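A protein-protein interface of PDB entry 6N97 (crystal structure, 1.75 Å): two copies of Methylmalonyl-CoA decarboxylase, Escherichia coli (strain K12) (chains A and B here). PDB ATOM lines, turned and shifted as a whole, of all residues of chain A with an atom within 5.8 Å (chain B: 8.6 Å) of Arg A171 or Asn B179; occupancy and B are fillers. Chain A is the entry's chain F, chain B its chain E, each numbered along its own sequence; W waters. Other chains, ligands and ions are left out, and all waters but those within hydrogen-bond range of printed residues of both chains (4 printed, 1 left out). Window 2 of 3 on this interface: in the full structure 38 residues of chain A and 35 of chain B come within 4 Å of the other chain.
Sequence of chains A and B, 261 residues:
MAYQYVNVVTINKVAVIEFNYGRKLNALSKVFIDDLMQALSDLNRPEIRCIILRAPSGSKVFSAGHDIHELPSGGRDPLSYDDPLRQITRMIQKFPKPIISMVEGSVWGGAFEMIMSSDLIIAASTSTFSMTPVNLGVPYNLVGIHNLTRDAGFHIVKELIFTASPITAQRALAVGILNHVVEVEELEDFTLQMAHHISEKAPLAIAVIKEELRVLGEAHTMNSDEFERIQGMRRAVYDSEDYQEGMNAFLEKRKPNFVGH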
ATOM      1  N   HIS A 155      -7.869  21.574  22.773  1.00  0.00           N
ATOM      2  CA  HIS A 155      -7.580  22.876  22.121  1.00  0.00           C
ATOM      3  C   HIS A 155      -8.899  23.622  22.015  1.00  0.00           C
ATOM      4  O   HIS A 155      -8.934  24.833  22.240  1.00  0.00           O
ATOM      5  CB  HIS A 155      -6.964  22.674  20.728  1.00  0.00           C
ATOM      6  CG  HIS A 155      -5.601  22.071  20.758  1.00  0.00           C
ATOM      7  ND1 HIS A 155      -5.134  21.259  19.742  1.00  0.00           N
ATOM      8  CD2 HIS A 155      -4.619  22.143  21.694  1.00  0.00           C
ATOM      9  CE1 HIS A 155      -3.908  20.845  20.033  1.00  0.00           C
ATOM     10  NE2 HIS A 155      -3.577  21.349  21.273  1.00  0.00           N
ATOM     11  N   ILE A 156      -9.967  22.921  21.701  1.00  0.00           N
ATOM     12  CA  ILE A 156     -11.308  23.545  21.495  1.00  0.00           C
ATOM     13  C   ILE A 156     -11.828  24.068  22.833  1.00  0.00           C
ATOM     14  O   ILE A 156     -12.318  25.201  22.883  1.00  0.00           O
ATOM     15  CB  ILE A 156     -12.300  22.588  20.826  1.00  0.00           C
ATOM     16  CG1 ILE A 156     -11.927  22.322  19.364  1.00  0.00           C
ATOM     17  CG2 ILE A 156     -13.705  23.158  20.929  1.00  0.00           C
ATOM     18  CD1 ILE A 156     -11.812  23.570  18.539  1.00  0.00           C
ATOM     19  N   LYS A 158     -10.062  24.868  25.485  1.00  0.00           N
ATOM     20  CA  LYS A 158      -9.219  26.033  25.885  1.00  0.00           C
ATOM     21  C   LYS A 158      -9.594  27.294  25.109  1.00  0.00           C
ATOM     22  O   LYS A 158      -9.667  28.370  25.737  1.00  0.00           O
ATOM     23  CB  LYS A 158      -7.736  25.701  25.749  1.00  0.00           C
ATOM     24  CG  LYS A 158      -7.314  24.735  26.832  1.00  0.00           C
ATOM     25  CD  LYS A 158      -5.992  24.129  26.440  1.00  0.00           C
ATOM     26  CE  LYS A 158      -5.389  23.241  27.466  1.00  0.00           C
ATOM     27  NZ  LYS A 158      -3.979  22.995  27.116  1.00  0.00           N
ATOM     28  N   GLU A 159      -9.896  27.186  23.816  1.00  0.00           N
ATOM     29  CA  GLU A 159     -10.417  28.378  23.087  1.00  0.00           C
ATOM     30  C   GLU A 159     -11.697  28.889  23.744  1.00  0.00           C
ATOM     31  O   GLU A 159     -11.802  30.105  23.977  1.00  0.00           O
ATOM     32  CB  GLU A 159     -10.569  28.090  21.601  1.00  0.00           C
ATOM     33  CG  GLU A 159     -11.200  29.261  20.846  1.00  0.00           C
ATOM     34  CD  GLU A 159     -11.484  28.972  19.387  1.00  0.00           C
ATOM     35  OE1 GLU A 159     -11.117  27.878  18.905  1.00  0.00           O
ATOM     36  OE2 GLU A 159     -12.207  29.806  18.777  1.00  0.00           O
ATOM     37  N   ILE A 167     -19.922  30.530  20.709  1.00  0.00           N
ATOM     38  CA  ILE A 167     -19.905  29.745  19.462  1.00  0.00           C
ATOM     39  C   ILE A 167     -21.340  29.510  19.021  1.00  0.00           C
ATOM     40  O   ILE A 167     -22.262  29.441  19.865  1.00  0.00           O
ATOM     41  CB  ILE A 167     -19.103  28.437  19.583  1.00  0.00           C
ATOM     42  CG1 ILE A 167     -19.715  27.492  20.603  1.00  0.00           C
ATOM     43  CG2 ILE A 167     -17.650  28.738  19.904  1.00  0.00           C
ATOM     44  CD1 ILE A 167     -19.112  26.109  20.510  1.00  0.00           C
ATOM     45  N   THR A 168     -21.485  29.316  17.728  1.00  0.00           N
ATOM     46  CA  THR A 168     -22.781  29.007  17.097  1.00  0.00           C
ATOM     47  C   THR A 168     -23.108  27.541  17.361  1.00  0.00           C
ATOM     48  O   THR A 168     -22.180  26.740  17.675  1.00  0.00           O
ATOM     49  CB  THR A 168     -22.715  29.278  15.591  1.00  0.00           C
ATOM     50  OG1 THR A 168     -21.818  28.360  14.974  1.00  0.00           O
ATOM     51  CG2 THR A 168     -22.303  30.697  15.289  1.00  0.00           C
ATOM     52  N   ALA A 169     -24.376  27.199  17.194  1.00  0.00           N
ATOM     53  CA  ALA A 169     -24.875  25.810  17.176  1.00  0.00           C
ATOM     54  C   ALA A 169     -24.151  24.994  16.121  1.00  0.00           C
ATOM     55  O   ALA A 169     -23.792  23.844  16.392  1.00  0.00           O
ATOM     56  CB  ALA A 169     -26.368  25.824  16.936  1.00  0.00           C
ATOM     57  N   GLN A 170     -23.859  25.576  14.944  1.00  0.00           N
ATOM     58  CA  GLN A 170     -23.198  24.831  13.854  1.00  0.00           C
ATOM     59  C   GLN A 170     -21.783  24.472  14.291  1.00  0.00           C
ATOM     60  O   GLN A 170     -21.355  23.324  14.048  1.00  0.00           O
ATOM     61  CB  GLN A 170     -23.189  25.638  12.564  1.00  0.00           C
ATOM     62  CG  GLN A 170     -24.597  25.842  11.977  1.00  0.00           C
ATOM     63  CD  GLN A 170     -25.426  26.843  12.753  1.00  0.00           C
ATOM     64  OE1 GLN A 170     -24.868  27.764  13.345  1.00  0.00           O
ATOM     65  NE2 GLN A 170     -26.756  26.727  12.692  1.00  0.00           N
ATOM     66  N   ARG A 171     -21.070  25.402  14.895  1.00  0.00           N
ATOM     67  CA  ARG A 171     -19.696  25.040  15.315  1.00  0.00           C
ATOM     68  C   ARG A 171     -19.767  24.080  16.505  1.00  0.00           C
ATOM     69  O   ARG A 171     -18.918  23.193  16.553  1.00  0.00           O
ATOM     70  CB  ARG A 171     -18.852  26.253  15.675  1.00  0.00           C
ATOM     71  CG  ARG A 171     -17.395  25.860  15.840  1.00  0.00           C
ATOM     72  CD  ARG A 171     -16.508  27.024  16.166  1.00  0.00           C
ATOM     73  NE  ARG A 171     -15.121  26.570  16.240  1.00  0.00           N
ATOM     74  CZ  ARG A 171     -14.198  27.195  16.961  1.00  0.00           C
ATOM     75  NH1 ARG A 171     -12.949  26.744  17.018  1.00  0.00           N
ATOM     76  NH2 ARG A 171     -14.539  28.271  17.657  1.00  0.00           N
ATOM     77  N   ALA A 172     -20.710  24.265  17.405  1.00  0.00           N
ATOM     78  CA  ALA A 172     -20.803  23.357  18.569  1.00  0.00           C
ATOM     79  C   ALA A 172     -21.110  21.934  18.074  1.00  0.00           C
ATOM     80  O   ALA A 172     -20.617  20.979  18.671  1.00  0.00           O
ATOM     81  CB  ALA A 172     -21.859  23.866  19.518  1.00  0.00           C
ATOM     82  N   LEU A 173     -21.899  21.781  16.995  1.00  0.00           N
ATOM     83  CA  LEU A 173     -22.149  20.440  16.396  1.00  0.00           C
ATOM     84  C   LEU A 173     -20.821  19.885  15.852  1.00  0.00           C
ATOM     85  O   LEU A 173     -20.502  18.658  16.033  1.00  0.00           O
ATOM     86  CB  LEU A 173     -23.180  20.597  15.272  1.00  0.00           C
ATOM     87  CG  LEU A 173     -23.576  19.311  14.558  1.00  0.00           C
ATOM     88  CD1 LEU A 173     -24.337  18.378  15.504  1.00  0.00           C
ATOM     89  CD2 LEU A 173     -24.375  19.625  13.291  1.00  0.00           C
ATOM     90  N   ALA A 174     -20.099  20.729  15.107  1.00  0.00           N
ATOM     91  CA  ALA A 174     -18.877  20.325  14.368  1.00  0.00           C
ATOM     92  C   ALA A 174     -17.824  19.805  15.361  1.00  0.00           C
ATOM     93  O   ALA A 174     -17.117  18.835  15.034  1.00  0.00           O
ATOM     94  CB  ALA A 174     -18.322  21.496  13.579  1.00  0.00           C
ATOM     95  N   VAL A 175     -17.716  20.435  16.526  1.00  0.00           N
ATOM     96  CA  VAL A 175     -16.612  20.094  17.465  1.00  0.00           C
ATOM     97  C   VAL A 175     -17.034  18.981  18.424  1.00  0.00           C
ATOM     98  O   VAL A 175     -16.171  18.558  19.204  1.00  0.00           O
ATOM     99  CB  VAL A 175     -16.084  21.363  18.170  1.00  0.00           C
ATOM    100  CG1 VAL A 175     -15.653  22.428  17.175  1.00  0.00           C
ATOM    101  CG2 VAL A 175     -17.041  21.946  19.188  1.00  0.00           C
ATOM    102  N   GLY A 176     -18.290  18.509  18.391  1.00  0.00           N
ATOM    103  CA  GLY A 176     -18.777  17.357  19.186  1.00  0.00           C
ATOM    104  C   GLY A 176     -19.528  17.704  20.468  1.00  0.00           C
ATOM    105  O   GLY A 176     -19.890  16.762  21.185  1.00  0.00           O
ATOM    106  N   ILE B  99      -0.542  29.688  25.388  1.00  0.00           N
ATOM    107  CA  ILE B  99       0.467  29.622  24.291  1.00  0.00           C
ATOM    108  C   ILE B  99      -0.234  29.155  23.000  1.00  0.00           C
ATOM    109  O   ILE B  99      -0.797  28.028  22.962  1.00  0.00           O
ATOM    110  CB  ILE B  99       1.663  28.745  24.707  1.00  0.00           C
ATOM    111  CG1 ILE B  99       2.372  29.339  25.925  1.00  0.00           C
ATOM    112  CG2 ILE B  99       2.595  28.591  23.525  1.00  0.00           C
ATOM    113  CD1 ILE B  99       3.488  28.508  26.474  1.00  0.00           C
ATOM    114  N   ILE B 100      -0.292  30.032  22.005  1.00  0.00           N
ATOM    115  CA  ILE B 100      -0.956  29.794  20.705  1.00  0.00           C
ATOM    116  C   ILE B 100       0.114  29.431  19.689  1.00  0.00           C
ATOM    117  O   ILE B 100       1.083  30.190  19.551  1.00  0.00           O
ATOM    118  CB  ILE B 100      -1.787  30.993  20.245  1.00  0.00           C
ATOM    119  CG1 ILE B 100      -2.816  31.370  21.313  1.00  0.00           C
ATOM    120  CG2 ILE B 100      -2.420  30.661  18.899  1.00  0.00           C
ATOM    121  CD1 ILE B 100      -3.509  32.657  21.041  1.00  0.00           C
ATOM    122  N   SER B 101       0.048  28.233  19.115  1.00  0.00           N
ATOM    123  CA  SER B 101       0.897  27.873  17.941  1.00  0.00           C
ATOM    124  C   SER B 101       0.238  28.435  16.696  1.00  0.00           C
ATOM    125  O   SER B 101      -0.854  27.982  16.339  1.00  0.00           O
ATOM    126  CB  SER B 101       1.088  26.410  17.815  1.00  0.00           C
ATOM    127  OG  SER B 101       1.830  25.922  18.915  1.00  0.00           O
ATOM    128  N   ILE B 115       3.408  21.486  19.039  1.00  0.00           N
ATOM    129  CA  ILE B 115       2.196  22.337  18.846  1.00  0.00           C
ATOM    130  C   ILE B 115       0.980  21.667  19.514  1.00  0.00           C
ATOM    131  O   ILE B 115       0.127  22.380  20.061  1.00  0.00           O
ATOM    132  CB  ILE B 115       1.969  22.730  17.373  1.00  0.00           C
ATOM    133  CG1 ILE B 115       1.638  21.558  16.462  1.00  0.00           C
ATOM    134  CG2 ILE B 115       3.165  23.516  16.843  1.00  0.00           C
ATOM    135  CD1 ILE B 115       1.060  21.997  15.121  1.00  0.00           C
ATOM    136  N   MET B 116       0.921  20.338  19.563  1.00  0.00           N
ATOM    137  CA  MET B 116      -0.213  19.662  20.225  1.00  0.00           C
ATOM    138  C   MET B 116      -0.167  19.970  21.729  1.00  0.00           C
ATOM    139  O   MET B 116      -1.247  20.079  22.304  1.00  0.00           O
ATOM    140  CB  MET B 116      -0.193  18.157  19.959  1.00  0.00           C
ATOM    141  CG  MET B 116      -0.435  17.857  18.503  1.00  0.00           C
ATOM    142  SD  MET B 116      -2.138  18.183  18.063  1.00  0.00           S
ATOM    143  CE  MET B 116      -2.888  16.667  18.643  1.00  0.00           C
ATOM    144  N   SER B 118       0.664  22.793  23.080  1.00  0.00           N
ATOM    145  CA  SER B 118       0.251  24.196  23.273  1.00  0.00           C
ATOM    146  C   SER B 118      -1.261  24.266  23.429  1.00  0.00           C
ATOM    147  O   SER B 118      -1.975  23.248  23.291  1.00  0.00           O
ATOM    148  CB  SER B 118       0.791  25.068  22.152  1.00  0.00           C
ATOM    149  OG  SER B 118       0.085  24.902  20.939  1.00  0.00           O
ATOM    150  N   ASP B 119      -1.782  25.440  23.758  1.00  0.00           N
ATOM    151  CA  ASP B 119      -3.206  25.585  24.161  1.00  0.00           C
ATOM    152  C   ASP B 119      -4.161  25.699  22.960  1.00  0.00           C
ATOM    153  O   ASP B 119      -5.293  25.149  23.072  1.00  0.00           O
ATOM    154  CB  ASP B 119      -3.303  26.760  25.122  1.00  0.00           C
ATOM    155  CG  ASP B 119      -2.408  26.565  26.324  1.00  0.00           C
ATOM    156  OD1 ASP B 119      -2.525  25.457  26.962  1.00  0.00           O
ATOM    157  OD2 ASP B 119      -1.573  27.453  26.597  1.00  0.00           O
ATOM    158  N   LEU B 120      -3.762  26.417  21.896  1.00  0.00           N
ATOM    159  CA  LEU B 120      -4.566  26.637  20.674  1.00  0.00           C
ATOM    160  C   LEU B 120      -3.614  26.486  19.480  1.00  0.00           C
ATOM    161  O   LEU B 120      -2.423  26.808  19.612  1.00  0.00           O
ATOM    162  CB  LEU B 120      -5.196  28.025  20.606  1.00  0.00           C
ATOM    163  CG  LEU B 120      -6.436  28.299  21.435  1.00  0.00           C
ATOM    164  CD1 LEU B 120      -6.066  28.481  22.886  1.00  0.00           C
ATOM    165  CD2 LEU B 120      -7.136  29.558  20.930  1.00  0.00           C
ATOM    166  N   ILE B 121      -4.112  25.980  18.369  1.00  0.00           N
ATOM    167  CA  ILE B 121      -3.391  25.940  17.075  1.00  0.00           C
ATOM    168  C   ILE B 121      -4.242  26.657  16.018  1.00  0.00           C
ATOM    169  O   ILE B 121      -5.394  26.292  15.760  1.00  0.00           O
ATOM    170  CB  ILE B 121      -3.022  24.531  16.635  1.00  0.00           C
ATOM    171  CG1 ILE B 121      -2.461  23.709  17.793  1.00  0.00           C
ATOM    172  CG2 ILE B 121      -2.075  24.612  15.455  1.00  0.00           C
ATOM    173  CD1 ILE B 121      -2.177  22.282  17.389  1.00  0.00           C
ATOM    174  N   ILE B 122      -3.672  27.701  15.453  1.00  0.00           N
ATOM    175  CA  ILE B 122      -4.264  28.450  14.314  1.00  0.00           C
ATOM    176  C   ILE B 122      -3.278  28.243  13.168  1.00  0.00           C
ATOM    177  O   ILE B 122      -2.065  28.518  13.360  1.00  0.00           O
ATOM    178  CB  ILE B 122      -4.494  29.925  14.684  1.00  0.00           C
ATOM    179  CG1 ILE B 122      -5.389  30.008  15.926  1.00  0.00           C
ATOM    180  CG2 ILE B 122      -5.092  30.664  13.501  1.00  0.00           C
ATOM    181  CD1 ILE B 122      -5.621  31.409  16.433  1.00  0.00           C
ATOM    182  N   ALA B 123      -3.782  27.807  12.025  1.00  0.00           N
ATOM    183  CA  ALA B 123      -2.931  27.354  10.914  1.00  0.00           C
ATOM    184  C   ALA B 123      -3.354  27.939   9.571  1.00  0.00           C
ATOM    185  O   ALA B 123      -4.545  28.154   9.324  1.00  0.00           O
ATOM    186  CB  ALA B 123      -2.911  25.853  10.837  1.00  0.00           C
ATOM    187  N   ASP B 151      -7.140  15.555  21.546  1.00  0.00           N
ATOM    188  CA  ASP B 151      -7.862  16.382  20.549  1.00  0.00           C
ATOM    189  C   ASP B 151      -8.645  15.478  19.592  1.00  0.00           C
ATOM    190  O   ASP B 151      -9.889  15.500  19.627  1.00  0.00           O
ATOM    191  CB  ASP B 151      -6.848  17.334  19.922  1.00  0.00           C
ATOM    192  CG  ASP B 151      -6.334  18.325  20.963  1.00  0.00           C
ATOM    193  OD1 ASP B 151      -7.135  19.227  21.409  1.00  0.00           O
ATOM    194  OD2 ASP B 151      -5.154  18.150  21.393  1.00  0.00           O
ATOM    195  N   ALA B 169      -4.376  20.908   6.612  1.00  0.00           N
ATOM    196  CA  ALA B 169      -4.967  21.769   7.647  1.00  0.00           C
ATOM    197  C   ALA B 169      -6.485  21.528   7.707  1.00  0.00           C
ATOM    198  O   ALA B 169      -7.046  21.550   8.805  1.00  0.00           O
ATOM    199  CB  ALA B 169      -4.605  23.209   7.384  1.00  0.00           C
ATOM    200  N   ALA B 172      -7.041  18.406   9.532  1.00  0.00           N
ATOM    201  CA  ALA B 172      -6.579  18.615  10.917  1.00  0.00           C
ATOM    202  C   ALA B 172      -7.664  19.383  11.676  1.00  0.00           C
ATOM    203  O   ALA B 172      -7.939  19.092  12.847  1.00  0.00           O
ATOM    204  CB  ALA B 172      -5.197  19.256  10.934  1.00  0.00           C
ATOM    205  N   LEU B 173      -8.379  20.276  10.994  1.00  0.00           N
ATOM    206  CA  LEU B 173      -9.492  21.023  11.603  1.00  0.00           C
ATOM    207  C   LEU B 173     -10.675  20.068  11.831  1.00  0.00           C
ATOM    208  O   LEU B 173     -11.268  20.082  12.929  1.00  0.00           O
ATOM    209  CB  LEU B 173      -9.891  22.146  10.655  1.00  0.00           C
ATOM    210  CG  LEU B 173     -11.044  23.010  11.139  1.00  0.00           C
ATOM    211  CD1 LEU B 173     -10.657  23.845  12.350  1.00  0.00           C
ATOM    212  CD2 LEU B 173     -11.530  23.881   9.988  1.00  0.00           C
ATOM    213  N   ALA B 174     -11.008  19.276  10.836  1.00  0.00           N
ATOM    214  CA  ALA B 174     -12.166  18.350  10.826  1.00  0.00           C
ATOM    215  C   ALA B 174     -12.022  17.351  11.976  1.00  0.00           C
ATOM    216  O   ALA B 174     -13.037  17.074  12.646  1.00  0.00           O
ATOM    217  CB  ALA B 174     -12.262  17.637   9.492  1.00  0.00           C
ATOM    218  N   GLY B 176     -10.299  17.690  14.830  1.00  0.00           N
ATOM    219  CA  GLY B 176     -10.264  18.362  16.130  1.00  0.00           C
ATOM    220  C   GLY B 176      -8.860  18.727  16.580  1.00  0.00           C
ATOM    221  O   GLY B 176      -8.733  19.222  17.707  1.00  0.00           O
ATOM    222  N   ILE B 177      -7.838  18.586  15.725  1.00  0.00           N
ATOM    223  CA  ILE B 177      -6.456  19.004  16.051  1.00  0.00           C
ATOM    224  C   ILE B 177      -6.339  20.530  16.065  1.00  0.00           C
ATOM    225  O   ILE B 177      -5.723  21.054  17.009  1.00  0.00           O
ATOM    226  CB  ILE B 177      -5.497  18.313  15.074  1.00  0.00           C
ATOM    227  CG1 ILE B 177      -5.414  16.819  15.418  1.00  0.00           C
ATOM    228  CG2 ILE B 177      -4.150  19.002  15.045  1.00  0.00           C
ATOM    229  CD1 ILE B 177      -4.815  15.981  14.327  1.00  0.00           C
ATOM    230  N   LEU B 178      -6.947  21.250  15.110  1.00  0.00           N
ATOM    231  CA  LEU B 178      -6.726  22.699  14.939  1.00  0.00           C
ATOM    232  C   LEU B 178      -7.941  23.435  15.472  1.00  0.00           C
ATOM    233  O   LEU B 178      -9.072  22.939  15.370  1.00  0.00           O
ATOM    234  CB  LEU B 178      -6.548  23.062  13.455  1.00  0.00           C
ATOM    235  CG  LEU B 178      -5.351  22.436  12.760  1.00  0.00           C
ATOM    236  CD1 LEU B 178      -5.306  22.887  11.321  1.00  0.00           C
ATOM    237  CD2 LEU B 178      -4.058  22.777  13.455  1.00  0.00           C
ATOM    238  N   ASN B 179      -7.722  24.651  15.930  1.00  0.00           N
ATOM    239  CA  ASN B 179      -8.836  25.546  16.283  1.00  0.00           C
ATOM    240  C   ASN B 179      -9.414  26.216  15.042  1.00  0.00           C
ATOM    241  O   ASN B 179     -10.675  26.340  14.929  1.00  0.00           O
ATOM    242  CB  ASN B 179      -8.351  26.590  17.276  1.00  0.00           C
ATOM    243  CG  ASN B 179      -8.053  25.937  18.600  1.00  0.00           C
ATOM    244  OD1 ASN B 179      -6.949  25.378  18.764  1.00  0.00           O
ATOM    245  ND2 ASN B 179      -9.017  26.030  19.507  1.00  0.00           N
ATOM    246  N   HIS B 180      -8.526  26.801  14.243  1.00  0.00           N
ATOM    247  CA  HIS B 180      -8.926  27.599  13.067  1.00  0.00           C
ATOM    248  C   HIS B 180      -7.937  27.383  11.934  1.00  0.00           C
ATOM    249  O   HIS B 180      -6.705  27.153  12.198  1.00  0.00           O
ATOM    250  CB  HIS B 180      -9.020  29.085  13.391  1.00  0.00           C
ATOM    251  CG  HIS B 180     -10.075  29.406  14.372  1.00  0.00           C
ATOM    252  ND1 HIS B 180     -11.406  29.590  14.014  1.00  0.00           N
ATOM    253  CD2 HIS B 180     -10.009  29.543  15.711  1.00  0.00           C
ATOM    254  CE1 HIS B 180     -12.086  29.859  15.110  1.00  0.00           C
ATOM    255  NE2 HIS B 180     -11.282  29.821  16.148  1.00  0.00           N
ATOM    256  N   VAL B 181      -8.475  27.438  10.729  1.00  0.00           N
ATOM    257  CA  VAL B 181      -7.698  27.448   9.465  1.00  0.00           C
ATOM    258  C   VAL B 181      -8.006  28.751   8.742  1.00  0.00           C
ATOM    259  O   VAL B 181      -9.148  29.044   8.578  1.00  0.00           O
ATOM    260  CB  VAL B 181      -7.989  26.257   8.567  1.00  0.00           C
ATOM    261  CG1 VAL B 181      -7.269  26.445   7.233  1.00  0.00           C
ATOM    262  CG2 VAL B 181      -7.568  24.950   9.254  1.00  0.00           C
ATOM    263  N   VAL B 182      -6.986  29.502   8.388  1.00  0.00           N
ATOM    264  CA  VAL B 182      -7.213  30.799   7.688  1.00  0.00           C
ATOM    265  C   VAL B 182      -6.228  30.924   6.530  1.00  0.00           C
ATOM    266  O   VAL B 182      -5.192  30.248   6.502  1.00  0.00           O
ATOM    267  CB  VAL B 182      -7.109  31.999   8.638  1.00  0.00           C
ATOM    268  CG1 VAL B 182      -8.107  31.921   9.799  1.00  0.00           C
ATOM    269  CG2 VAL B 182      -5.697  32.134   9.134  1.00  0.00           C
ATOM    270  N   PHE B 190      -5.370  37.463  12.269  1.00  0.00           N
ATOM    271  CA  PHE B 190      -6.441  36.644  12.913  1.00  0.00           C
ATOM    272  C   PHE B 190      -5.953  36.187  14.289  1.00  0.00           C
ATOM    273  O   PHE B 190      -6.681  36.337  15.271  1.00  0.00           O
ATOM    274  CB  PHE B 190      -6.826  35.455  12.030  1.00  0.00           C
ATOM    275  CG  PHE B 190      -7.915  34.598  12.609  1.00  0.00           C
ATOM    276  CD1 PHE B 190      -7.601  33.620  13.545  1.00  0.00           C
ATOM    277  CD2 PHE B 190      -9.234  34.763  12.238  1.00  0.00           C
ATOM    278  CE1 PHE B 190      -8.594  32.831  14.102  1.00  0.00           C
ATOM    279  CE2 PHE B 190     -10.223  33.953  12.783  1.00  0.00           C
ATOM    280  CZ  PHE B 190      -9.904  32.995  13.726  1.00  0.00           C
ATOM    281  N   MET B 194      -7.181  37.405  18.251  1.00  0.00           N
ATOM    282  CA  MET B 194      -7.604  36.472  19.319  1.00  0.00           C
ATOM    283  C   MET B 194      -6.708  36.649  20.561  1.00  0.00           C
ATOM    284  O   MET B 194      -7.275  36.641  21.678  1.00  0.00           O
ATOM    285  CB  MET B 194      -7.610  35.026  18.818  1.00  0.00           C
ATOM    286  CG  MET B 194      -8.360  34.115  19.790  1.00  0.00           C
ATOM    287  SD  MET B 194      -8.527  32.470  19.140  1.00  0.00           S
ATOM    288  CE  MET B 194      -9.902  32.738  18.024  1.00  0.00           C
HETATM  289  O   HOH W   1      -9.399  20.125  20.211  1.00  0.00           O
HETATM  290  O   HOH W   2      -3.965  19.090  23.704  1.00  0.00           O
HETATM  291  O   HOH W   3      -0.756  23.632  27.242  1.00  0.00           O
HETATM  292  O   HOH W   4      -3.218  21.430  24.926  1.00  0.00           O
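His A155 touches Asp B119.
Ile B121 touches His A155.
Ile A156 touches Asn B179 (CD1 to ND2, 3.8 Å).
Leu B120 touches Glu A159.
OE2 of Glu A159 touches CE of Met B194, 3.8 Å away.
Arg A171 touches His B180 (NH1 to NE2, 3.6 Å).
Water W3 lies within hydrogen-bond range of the side-chain carboxylate of Asp B119 (2.6 Å) and the side-chain amino group of Lys A158 (3.3 Å).
Water W1 lies within hydrogen-bond range of the side-chain carboxylate (OD1) of Asp B151 (2.7 Å), the backbone carbonyl oxygen (O) of Gly B176 (2.7 Å), the backbone NH (N) of Ile A156 (3.2 Å) and the backbone NH (N) of His A155 (3.3 Å).
Water W4 lies within hydrogen-bond range of the backbone carbonyl oxygen of Ser B118 (2.7 Å) and the side-chain amino group of Lys A158 (2.8 Å).
Water W2 lies within hydrogen-bond range of OD2 of Asp B151 (2.8 Å), O of Met B116 (3.2 Å) and NE2 of His A155 (3.3 Å).
OG1 of Thr A168 sits at hydrogen-bond distance from N of Arg A171 (3.1 Å).
The backbone NH (N) of Ile B177 is in hydrogen-bond range of the backbone carbonyl oxygen (O) of Ala B172, at 2.9 Å.
OG of Ser B101 sits at hydrogen-bond distance from OG of Ser B118.
The side-chain carboxylate (OD2) of Asp B119 lies within hydrogen-bond range of the backbone NH (N) of Ile B99, 2.7 Å away.
The side-chain hydroxyl of Ser B118 sits at hydrogen-bond distance from the backbone carbonyl oxygen of Leu B120 (3.4 Å).
The backbone carbonyl oxygen of Ile B121 sits at hydrogen-bond distance from the backbone NH of Asn B179, 2.9 Å away.
Hydrophobic or aromatic side chains of chain A within 4 Å of the printed part of chain B: His A155 and Ile A156.
Hydrophobic or aromatic side chains of chain B within 4 Å of the printed part of chain A: Met B116, Leu B120, Ile B121, His B180 and Met B194.
5 positions are printed for both chains.
Of the 15 pairs that touch across the chains among the printed residues, none has its exchanged pair printed and touching as well.
The backbone carbonyl oxygen (O) of Ile B177 is in hydrogen-bond range of a ring nitrogen (ND1) of His A155, 2.8 Å away.
The backbone carbonyl oxygen of Met B116 sits at hydrogen-bond distance from a ring nitrogen (NE2) of His A155 (2.8 Å).
OD1 of Asp B119 lies within salt-bridge range of NZ of Lys A158 (2.9 Å).
OE2 of Glu A159 sits at hydrogen-bond distance from NE2 of His B180 (2.8 Å).
ND2 of Asn B179 lies within hydrogen-bond range of O of His A155 (3.0 Å).
O of Ser B118 sits at hydrogen-bond distance from NE2 of His A155, 3.2 Å away.
The guanidinium group (NH1) of Arg A171 sits at hydrogen-bond distance from the backbone carbonyl oxygen (O) of Asn B179, at 3.1 Å.
ND2 of Asn B179 lies within hydrogen-bond range of OE1 of Glu A159.
OD1 of Asp B151 is in hydrogen-bond range of N of His A155.
Of the printed residues of chain B, Ile A156 touches Asn B179 (3.8 Å).
Of the printed residues of chain B, Arg A171 touches Asn B179 and His B180.
Ile B115 touches none of the printed residues of chain A.
Printed residues of chain A within 4 Å of Asp B119: His A155 (3.4 Å) and Lys A158 (2.9 Å).
The nearest printed residue of chain B that does not touch Arg A171 is Leu B178 (5.7 Å).
The nearest printed residue of chain A that does not touch Ile B177 is Ile A156 (6.6 Å).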
